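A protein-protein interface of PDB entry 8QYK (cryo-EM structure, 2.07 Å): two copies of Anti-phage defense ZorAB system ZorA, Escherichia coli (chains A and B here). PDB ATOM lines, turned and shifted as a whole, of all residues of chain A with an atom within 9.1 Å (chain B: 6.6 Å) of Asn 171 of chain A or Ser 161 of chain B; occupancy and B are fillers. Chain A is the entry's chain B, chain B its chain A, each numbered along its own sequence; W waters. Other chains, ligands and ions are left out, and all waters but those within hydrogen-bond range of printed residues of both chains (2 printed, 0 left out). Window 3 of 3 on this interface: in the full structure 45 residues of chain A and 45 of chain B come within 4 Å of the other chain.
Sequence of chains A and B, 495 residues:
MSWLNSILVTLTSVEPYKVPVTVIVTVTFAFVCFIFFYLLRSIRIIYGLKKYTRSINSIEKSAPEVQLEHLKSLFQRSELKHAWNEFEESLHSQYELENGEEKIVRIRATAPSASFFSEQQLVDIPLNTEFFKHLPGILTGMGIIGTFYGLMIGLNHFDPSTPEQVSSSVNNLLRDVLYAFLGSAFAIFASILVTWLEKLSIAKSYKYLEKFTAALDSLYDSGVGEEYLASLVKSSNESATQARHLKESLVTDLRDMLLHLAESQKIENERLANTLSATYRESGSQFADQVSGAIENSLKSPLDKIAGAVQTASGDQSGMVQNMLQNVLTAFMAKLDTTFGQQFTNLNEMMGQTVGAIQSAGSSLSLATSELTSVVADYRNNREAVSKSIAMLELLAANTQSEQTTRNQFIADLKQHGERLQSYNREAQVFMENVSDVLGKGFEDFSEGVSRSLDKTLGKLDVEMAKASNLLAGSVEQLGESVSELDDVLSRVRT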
ATOM      1  N   GLY A 154      18.533  21.120   5.916  1.00  0.00           N
ATOM      2  CA  GLY A 154      18.580  19.713   6.275  1.00  0.00           C
ATOM      3  C   GLY A 154      19.978  19.232   6.599  1.00  0.00           C
ATOM      4  O   GLY A 154      20.189  18.521   7.585  1.00  0.00           O
ATOM      5  N   PHE A 158      21.909  17.931  10.177  1.00  0.00           N
ATOM      6  CA  PHE A 158      22.434  16.571  10.160  1.00  0.00           C
ATOM      7  C   PHE A 158      23.740  16.518  10.941  1.00  0.00           C
ATOM      8  O   PHE A 158      24.746  17.097  10.519  1.00  0.00           O
ATOM      9  CB  PHE A 158      22.643  16.103   8.720  1.00  0.00           C
ATOM     10  CG  PHE A 158      23.247  14.734   8.605  1.00  0.00           C
ATOM     11  CD1 PHE A 158      22.476  13.601   8.799  1.00  0.00           C
ATOM     12  CD2 PHE A 158      24.583  14.582   8.286  1.00  0.00           C
ATOM     13  CE1 PHE A 158      23.028  12.345   8.686  1.00  0.00           C
ATOM     14  CE2 PHE A 158      25.141  13.329   8.173  1.00  0.00           C
ATOM     15  CZ  PHE A 158      24.362  12.208   8.372  1.00  0.00           C
ATOM     16  N   GLU A 164      24.112   5.395  17.582  1.00  0.00           N
ATOM     17  CA  GLU A 164      22.679   5.165  17.707  1.00  0.00           C
ATOM     18  C   GLU A 164      21.840   6.293  17.124  1.00  0.00           C
ATOM     19  O   GLU A 164      20.636   6.104  16.922  1.00  0.00           O
ATOM     20  CB  GLU A 164      22.317   4.958  19.178  1.00  0.00           C
ATOM     21  CG  GLU A 164      22.675   3.580  19.706  1.00  0.00           C
ATOM     22  CD  GLU A 164      24.128   3.480  20.130  1.00  0.00           C
ATOM     23  OE1 GLU A 164      24.726   4.523  20.465  1.00  0.00           O
ATOM     24  OE2 GLU A 164      24.674   2.357  20.128  1.00  0.00           O
ATOM     25  N   GLN A 165      22.434   7.450  16.847  1.00  0.00           N
ATOM     26  CA  GLN A 165      21.720   8.577  16.268  1.00  0.00           C
ATOM     27  C   GLN A 165      21.745   8.576  14.746  1.00  0.00           C
ATOM     28  O   GLN A 165      21.212   9.504  14.131  1.00  0.00           O
ATOM     29  CB  GLN A 165      22.305   9.894  16.787  1.00  0.00           C
ATOM     30  CG  GLN A 165      22.062  10.153  18.262  1.00  0.00           C
ATOM     31  CD  GLN A 165      22.818  11.365  18.771  1.00  0.00           C
ATOM     32  OE1 GLN A 165      23.855  11.739  18.223  1.00  0.00           O
ATOM     33  NE2 GLN A 165      22.301  11.986  19.824  1.00  0.00           N
ATOM     34  N   VAL A 166      22.349   7.561  14.126  1.00  0.00           N
ATOM     35  CA  VAL A 166      22.553   7.581  12.681  1.00  0.00           C
ATOM     36  C   VAL A 166      21.230   7.439  11.935  1.00  0.00           C
ATOM     37  O   VAL A 166      20.947   8.203  11.004  1.00  0.00           O
ATOM     38  CB  VAL A 166      23.555   6.487  12.275  1.00  0.00           C
ATOM     39  CG1 VAL A 166      23.599   6.336  10.765  1.00  0.00           C
ATOM     40  CG2 VAL A 166      24.925   6.817  12.817  1.00  0.00           C
ATOM     41  N   SER A 167      20.404   6.463  12.323  1.00  0.00           N
ATOM     42  CA  SER A 167      19.160   6.215  11.598  1.00  0.00           C
ATOM     43  C   SER A 167      18.205   7.397  11.701  1.00  0.00           C
ATOM     44  O   SER A 167      17.590   7.799  10.705  1.00  0.00           O
ATOM     45  CB  SER A 167      18.493   4.943  12.120  1.00  0.00           C
ATOM     46  OG  SER A 167      19.298   3.808  11.869  1.00  0.00           O
ATOM     47  N   SER A 168      18.069   7.966  12.901  1.00  0.00           N
ATOM     48  CA  SER A 168      17.208   9.129  13.081  1.00  0.00           C
ATOM     49  C   SER A 168      17.710  10.315  12.266  1.00  0.00           C
ATOM     50  O   SER A 168      16.914  11.047  11.666  1.00  0.00           O
ATOM     51  CB  SER A 168      17.132   9.494  14.563  1.00  0.00           C
ATOM     52  OG  SER A 168      16.522   8.459  15.312  1.00  0.00           O
ATOM     53  N   SER A 169      19.027  10.528  12.250  1.00  0.00           N
ATOM     54  CA  SER A 169      19.593  11.628  11.477  1.00  0.00           C
ATOM     55  C   SER A 169      19.331  11.450   9.989  1.00  0.00           C
ATOM     56  O   SER A 169      18.964  12.407   9.296  1.00  0.00           O
ATOM     57  CB  SER A 169      21.093  11.736  11.744  1.00  0.00           C
ATOM     58  OG  SER A 169      21.339  12.164  13.070  1.00  0.00           O
ATOM     59  N   VAL A 170      19.500  10.228   9.485  1.00  0.00           N
ATOM     60  CA  VAL A 170      19.231   9.956   8.078  1.00  0.00           C
ATOM     61  C   VAL A 170      17.759  10.197   7.763  1.00  0.00           C
ATOM     62  O   VAL A 170      17.419  10.784   6.729  1.00  0.00           O
ATOM     63  CB  VAL A 170      19.669   8.523   7.719  1.00  0.00           C
ATOM     64  CG1 VAL A 170      19.156   8.130   6.344  1.00  0.00           C
ATOM     65  CG2 VAL A 170      21.181   8.408   7.772  1.00  0.00           C
ATOM     66  N   ASN A 171      16.866   9.760   8.653  1.00  0.00           N
ATOM     67  CA  ASN A 171      15.438   9.957   8.423  1.00  0.00           C
ATOM     68  C   ASN A 171      15.073  11.439   8.385  1.00  0.00           C
ATOM     69  O   ASN A 171      14.344  11.882   7.488  1.00  0.00           O
ATOM     70  CB  ASN A 171      14.636   9.227   9.498  1.00  0.00           C
ATOM     71  CG  ASN A 171      14.689   7.722   9.332  1.00  0.00           C
ATOM     72  OD1 ASN A 171      15.287   7.213   8.387  1.00  0.00           O
ATOM     73  ND2 ASN A 171      14.063   7.003  10.254  1.00  0.00           N
ATOM     74  N   ASN A 172      15.580  12.224   9.340  1.00  0.00           N
ATOM     75  CA  ASN A 172      15.293  13.657   9.338  1.00  0.00           C
ATOM     76  C   ASN A 172      15.856  14.333   8.095  1.00  0.00           C
ATOM     77  O   ASN A 172      15.207  15.208   7.503  1.00  0.00           O
ATOM     78  CB  ASN A 172      15.836  14.313  10.607  1.00  0.00           C
ATOM     79  CG  ASN A 172      15.390  13.602  11.871  1.00  0.00           C
ATOM     80  OD1 ASN A 172      14.327  12.988  11.906  1.00  0.00           O
ATOM     81  ND2 ASN A 172      16.205  13.683  12.916  1.00  0.00           N
ATOM     82  N   LEU A 173      17.062  13.940   7.677  1.00  0.00           N
ATOM     83  CA  LEU A 173      17.643  14.535   6.480  1.00  0.00           C
ATOM     84  C   LEU A 173      16.821  14.204   5.241  1.00  0.00           C
ATOM     85  O   LEU A 173      16.629  15.061   4.372  1.00  0.00           O
ATOM     86  CB  LEU A 173      19.096  14.084   6.327  1.00  0.00           C
ATOM     87  CG  LEU A 173      19.944  14.732   5.230  1.00  0.00           C
ATOM     88  CD1 LEU A 173      21.387  14.689   5.639  1.00  0.00           C
ATOM     89  CD2 LEU A 173      19.791  14.007   3.904  1.00  0.00           C
ATOM     90  N   LEU A 174      16.320  12.971   5.143  1.00  0.00           N
ATOM     91  CA  LEU A 174      15.483  12.613   4.001  1.00  0.00           C
ATOM     92  C   LEU A 174      14.165  13.383   4.017  1.00  0.00           C
ATOM     93  O   LEU A 174      13.661  13.781   2.960  1.00  0.00           O
ATOM     94  CB  LEU A 174      15.245  11.104   3.978  1.00  0.00           C
ATOM     95  CG  LEU A 174      16.498  10.256   3.730  1.00  0.00           C
ATOM     96  CD1 LEU A 174      16.170   8.773   3.707  1.00  0.00           C
ATOM     97  CD2 LEU A 174      17.217  10.674   2.452  1.00  0.00           C
ATOM     98  N   ARG A 175      13.607  13.631   5.207  1.00  0.00           N
ATOM     99  CA  ARG A 175      12.418  14.481   5.303  1.00  0.00           C
ATOM    100  C   ARG A 175      12.693  15.894   4.794  1.00  0.00           C
ATOM    101  O   ARG A 175      11.871  16.486   4.076  1.00  0.00           O
ATOM    102  CB  ARG A 175      11.930  14.541   6.751  1.00  0.00           C
ATOM    103  CG  ARG A 175      11.498  13.219   7.349  1.00  0.00           C
ATOM    104  CD  ARG A 175      10.252  12.674   6.676  1.00  0.00           C
ATOM    105  NE  ARG A 175       9.101  13.544   6.889  1.00  0.00           N
ATOM    106  CZ  ARG A 175       7.984  13.495   6.176  1.00  0.00           C
ATOM    107  NH1 ARG A 175       7.823  12.613   5.204  1.00  0.00           N
ATOM    108  NH2 ARG A 175       7.004  14.353   6.447  1.00  0.00           N
ATOM    109  N   ASP A 176      13.830  16.469   5.184  1.00  0.00           N
ATOM    110  CA  ASP A 176      14.150  17.819   4.727  1.00  0.00           C
ATOM    111  C   ASP A 176      14.380  17.851   3.218  1.00  0.00           C
ATOM    112  O   ASP A 176      13.986  18.810   2.533  1.00  0.00           O
ATOM    113  CB  ASP A 176      15.361  18.352   5.491  1.00  0.00           C
ATOM    114  CG  ASP A 176      15.122  18.396   6.988  1.00  0.00           C
ATOM    115  OD1 ASP A 176      15.968  18.948   7.718  1.00  0.00           O
ATOM    116  OD2 ASP A 176      14.078  17.882   7.439  1.00  0.00           O
ATOM    117  N   VAL A 177      15.003  16.799   2.681  1.00  0.00           N
ATOM    118  CA  VAL A 177      15.127  16.673   1.234  1.00  0.00           C
ATOM    119  C   VAL A 177      13.748  16.656   0.591  1.00  0.00           C
ATOM    120  O   VAL A 177      13.537  17.241  -0.475  1.00  0.00           O
ATOM    121  CB  VAL A 177      15.937  15.415   0.866  1.00  0.00           C
ATOM    122  CG1 VAL A 177      15.924  15.203  -0.637  1.00  0.00           C
ATOM    123  CG2 VAL A 177      17.362  15.536   1.365  1.00  0.00           C
ATOM    124  N   LEU A 178      12.791  15.984   1.234  1.00  0.00           N
ATOM    125  CA  LEU A 178      11.425  15.943   0.724  1.00  0.00           C
ATOM    126  C   LEU A 178      10.806  17.338   0.666  1.00  0.00           C
ATOM    127  O   LEU A 178      10.146  17.690  -0.317  1.00  0.00           O
ATOM    128  CB  LEU A 178      10.588  15.007   1.596  1.00  0.00           C
ATOM    129  CG  LEU A 178       9.163  14.633   1.203  1.00  0.00           C
ATOM    130  CD1 LEU A 178       8.856  13.293   1.801  1.00  0.00           C
ATOM    131  CD2 LEU A 178       8.171  15.652   1.706  1.00  0.00           C
ATOM    132  N   TYR A 179      11.003  18.140   1.714  1.00  0.00           N
ATOM    133  CA  TYR A 179      10.552  19.538   1.684  1.00  0.00           C
ATOM    134  C   TYR A 179      11.119  20.286   0.473  1.00  0.00           C
ATOM    135  O   TYR A 179      10.379  20.926  -0.305  1.00  0.00           O
ATOM    136  CB  TYR A 179      10.983  20.245   2.973  1.00  0.00           C
ATOM    137  CG  TYR A 179      10.141  19.970   4.196  1.00  0.00           C
ATOM    138  CD1 TYR A 179       8.762  20.066   4.152  1.00  0.00           C
ATOM    139  CD2 TYR A 179      10.732  19.614   5.401  1.00  0.00           C
ATOM    140  CE1 TYR A 179       7.995  19.830   5.275  1.00  0.00           C
ATOM    141  CE2 TYR A 179       9.969  19.365   6.526  1.00  0.00           C
ATOM    142  CZ  TYR A 179       8.600  19.472   6.454  1.00  0.00           C
ATOM    143  OH  TYR A 179       7.827  19.229   7.564  1.00  0.00           O
ATOM    144  N   LEU B 155      10.972   8.955  -0.628  1.00  0.00           N
ATOM    145  CA  LEU B 155      11.574   9.493   0.584  1.00  0.00           C
ATOM    146  C   LEU B 155      10.572   9.564   1.727  1.00  0.00           C
ATOM    147  O   LEU B 155      10.956   9.410   2.890  1.00  0.00           O
ATOM    148  CB  LEU B 155      12.170  10.871   0.307  1.00  0.00           C
ATOM    149  CG  LEU B 155      13.387  10.872  -0.617  1.00  0.00           C
ATOM    150  CD1 LEU B 155      13.832  12.289  -0.902  1.00  0.00           C
ATOM    151  CD2 LEU B 155      14.521  10.057  -0.024  1.00  0.00           C
ATOM    152  N   PHE B 158      10.245   6.184   3.310  1.00  0.00           N
ATOM    153  CA  PHE B 158      11.460   5.747   3.989  1.00  0.00           C
ATOM    154  C   PHE B 158      11.494   6.359   5.383  1.00  0.00           C
ATOM    155  O   PHE B 158      11.984   7.472   5.579  1.00  0.00           O
ATOM    156  CB  PHE B 158      12.702   6.121   3.188  1.00  0.00           C
ATOM    157  CG  PHE B 158      13.894   5.268   3.505  1.00  0.00           C
ATOM    158  CD1 PHE B 158      14.639   5.495   4.648  1.00  0.00           C
ATOM    159  CD2 PHE B 158      14.260   4.230   2.670  1.00  0.00           C
ATOM    160  CE1 PHE B 158      15.729   4.709   4.947  1.00  0.00           C
ATOM    161  CE2 PHE B 158      15.348   3.439   2.965  1.00  0.00           C
ATOM    162  CZ  PHE B 158      16.085   3.679   4.105  1.00  0.00           C
ATOM    163  N   ASP B 159      10.967   5.623   6.353  1.00  0.00           N
ATOM    164  CA  ASP B 159      11.036   5.991   7.760  1.00  0.00           C
ATOM    165  C   ASP B 159      10.958   4.709   8.578  1.00  0.00           C
ATOM    166  O   ASP B 159       9.961   4.473   9.273  1.00  0.00           O
ATOM    167  CB  ASP B 159       9.905   6.956   8.127  1.00  0.00           C
ATOM    168  CG  ASP B 159      10.086   7.589   9.499  1.00  0.00           C
ATOM    169  OD1 ASP B 159      10.801   7.017  10.349  1.00  0.00           O
ATOM    170  OD2 ASP B 159       9.504   8.670   9.729  1.00  0.00           O
ATOM    171  N   PRO B 160      11.981   3.849   8.515  1.00  0.00           N
ATOM    172  CA  PRO B 160      11.891   2.545   9.187  1.00  0.00           C
ATOM    173  C   PRO B 160      11.850   2.649  10.703  1.00  0.00           C
ATOM    174  O   PRO B 160      10.990   2.035  11.343  1.00  0.00           O
ATOM    175  CB  PRO B 160      13.150   1.815   8.702  1.00  0.00           C
ATOM    176  CG  PRO B 160      14.107   2.901   8.355  1.00  0.00           C
ATOM    177  CD  PRO B 160      13.280   4.042   7.844  1.00  0.00           C
ATOM    178  N   SER B 161      12.778   3.409  11.287  1.00  0.00           N
ATOM    179  CA  SER B 161      12.850   3.635  12.731  1.00  0.00           C
ATOM    180  C   SER B 161      12.967   2.335  13.523  1.00  0.00           C
ATOM    181  O   SER B 161      12.728   2.320  14.734  1.00  0.00           O
ATOM    182  CB  SER B 161      11.644   4.444  13.225  1.00  0.00           C
ATOM    183  OG  SER B 161      11.675   5.766  12.716  1.00  0.00           O
ATOM    184  N   THR B 162      13.333   1.242  12.857  1.00  0.00           N
ATOM    185  CA  THR B 162      13.465  -0.068  13.479  1.00  0.00           C
ATOM    186  C   THR B 162      14.318  -0.955  12.583  1.00  0.00           C
ATOM    187  O   THR B 162      14.042  -1.068  11.381  1.00  0.00           O
ATOM    188  CB  THR B 162      12.092  -0.704  13.715  1.00  0.00           C
ATOM    189  OG1 THR B 162      11.396   0.020  14.738  1.00  0.00           O
ATOM    190  CG2 THR B 162      12.236  -2.159  14.141  1.00  0.00           C
ATOM    191  N   PRO B 163      15.360  -1.594  13.121  1.00  0.00           N
ATOM    192  CA  PRO B 163      16.235  -2.414  12.265  1.00  0.00           C
ATOM    193  C   PRO B 163      15.517  -3.564  11.585  1.00  0.00           C
ATOM    194  O   PRO B 163      15.973  -4.033  10.534  1.00  0.00           O
ATOM    195  CB  PRO B 163      17.309  -2.914  13.244  1.00  0.00           C
ATOM    196  CG  PRO B 163      16.678  -2.807  14.592  1.00  0.00           C
ATOM    197  CD  PRO B 163      15.796  -1.600  14.526  1.00  0.00           C
ATOM    198  N   GLN B 165      12.475  -3.499  10.158  1.00  0.00           N
ATOM    199  CA  GLN B 165      11.694  -3.053   9.012  1.00  0.00           C
ATOM    200  C   GLN B 165      12.486  -2.164   8.059  1.00  0.00           C
ATOM    201  O   GLN B 165      11.888  -1.435   7.261  1.00  0.00           O
ATOM    202  CB  GLN B 165      10.432  -2.330   9.486  1.00  0.00           C
ATOM    203  CG  GLN B 165      10.693  -1.058  10.266  1.00  0.00           C
ATOM    204  CD  GLN B 165       9.468  -0.578  11.021  1.00  0.00           C
ATOM    205  OE1 GLN B 165       8.798   0.367  10.604  1.00  0.00           O
ATOM    206  NE2 GLN B 165       9.170  -1.226  12.140  1.00  0.00           N
ATOM    207  N   VAL B 166      13.818  -2.206   8.124  1.00  0.00           N
ATOM    208  CA  VAL B 166      14.621  -1.443   7.174  1.00  0.00           C
ATOM    209  C   VAL B 166      14.488  -2.028   5.772  1.00  0.00           C
ATOM    210  O   VAL B 166      14.440  -1.292   4.780  1.00  0.00           O
ATOM    211  CB  VAL B 166      16.090  -1.391   7.631  1.00  0.00           C
ATOM    212  CG1 VAL B 166      16.940  -0.661   6.606  1.00  0.00           C
ATOM    213  CG2 VAL B 166      16.199  -0.713   8.985  1.00  0.00           C
HETATM  214  O   HOH W   1      16.204   2.272  11.743  1.00  0.00           O
HETATM  215  O   HOH W   2      13.792   7.883  12.709  1.00  0.00           O
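ND2 of Asn 171 of chain A sits at hydrogen-bond distance from OD1 of Asp 159 of chain B (3.3 Å).
The side-chain carboxylate (OD1) of Asp 159 of chain B sits at hydrogen-bond distance from the side-chain hydroxyl (OG) of Ser 161 of chain B, 2.8 Å away. The side-chain amide oxygen (OE1) of Gln 165 of chain B sits close to the backbone carbonyl oxygen (O) of Pro 160 of chain B, 2.9 Å away. The backbone carbonyl oxygen of Ser 167 of chain A sits close to the side-chain amide oxygen of Asn 171 of chain A.
Pro 160 of chain B touches Asn 171 of chain A (CD to OD1, 3.8 Å). Asn 171 of chain A touches Ser 161 of chain B (ND2 to OG, 3.6 Å). Leu 155 of chain B touches Leu 174 of chain A. Phe 158 of chain B touches Leu 174 of chain A. Val 177 of chain A touches Leu 155 of chain B.
Of chain B, only Asp 159, Pro 160 and Ser 161 come within 4 Å of Asn 171 of chain A. Of chain A, only Asn 171 (3.6 Å) comes within 4 Å of Ser 161 of chain B. Of the printed residues of chain A, Asp 159 of chain B touches Asn 171. Of chain A, only Asn 171 comes within 4 Å of Pro 160 of chain B. Thr 162 of chain B touches none of the printed residues of chain A. Of the printed residues of chain B, Leu 174 of chain A touches Leu 155 and Phe 158. Printed residues of chain A within 4 Å of Leu 155 of chain B: Leu 174 (3.7 Å) and Val 177 (3.6 Å). The nearest residue of chain B that does not touch Asn 171 of chain A is Phe 158 of chain B (4.2 Å). The nearest residue of chain A that does not touch Ser 161 of chain B is Ser 167 of chain A (5.8 Å).
Of the 9 printed residues of chain B, 5 touch a printed residue of chain A. Hydrophobic or aromatic side chains of chain B within 4 Å of the printed part of chain A: Leu 155, Phe 158 and Pro 160. Of the 18 printed residues of chain A, 3 touch a printed residue of chain B. Hydrophobic or aromatic side chains of chain A that line the printed part of chain B: Leu 174 and Val 177.
3 positions are printed for both chains. Of the 6 pairs that touch across the chains among the printed residues, none has its exchanged pair printed and touching as well.
Water W2 bridges the side-chain amide nitrogen (ND2) of Asn 171 of chain A (2.6 Å) and the side-chain hydroxyl (OG) of Ser 161 of chain B (3.0 Å). Water W1 bridges the backbone NH of Thr 162 of chain B (3.2 Å) and the side-chain hydroxyl of Ser 167 of chain A (3.5 Å).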
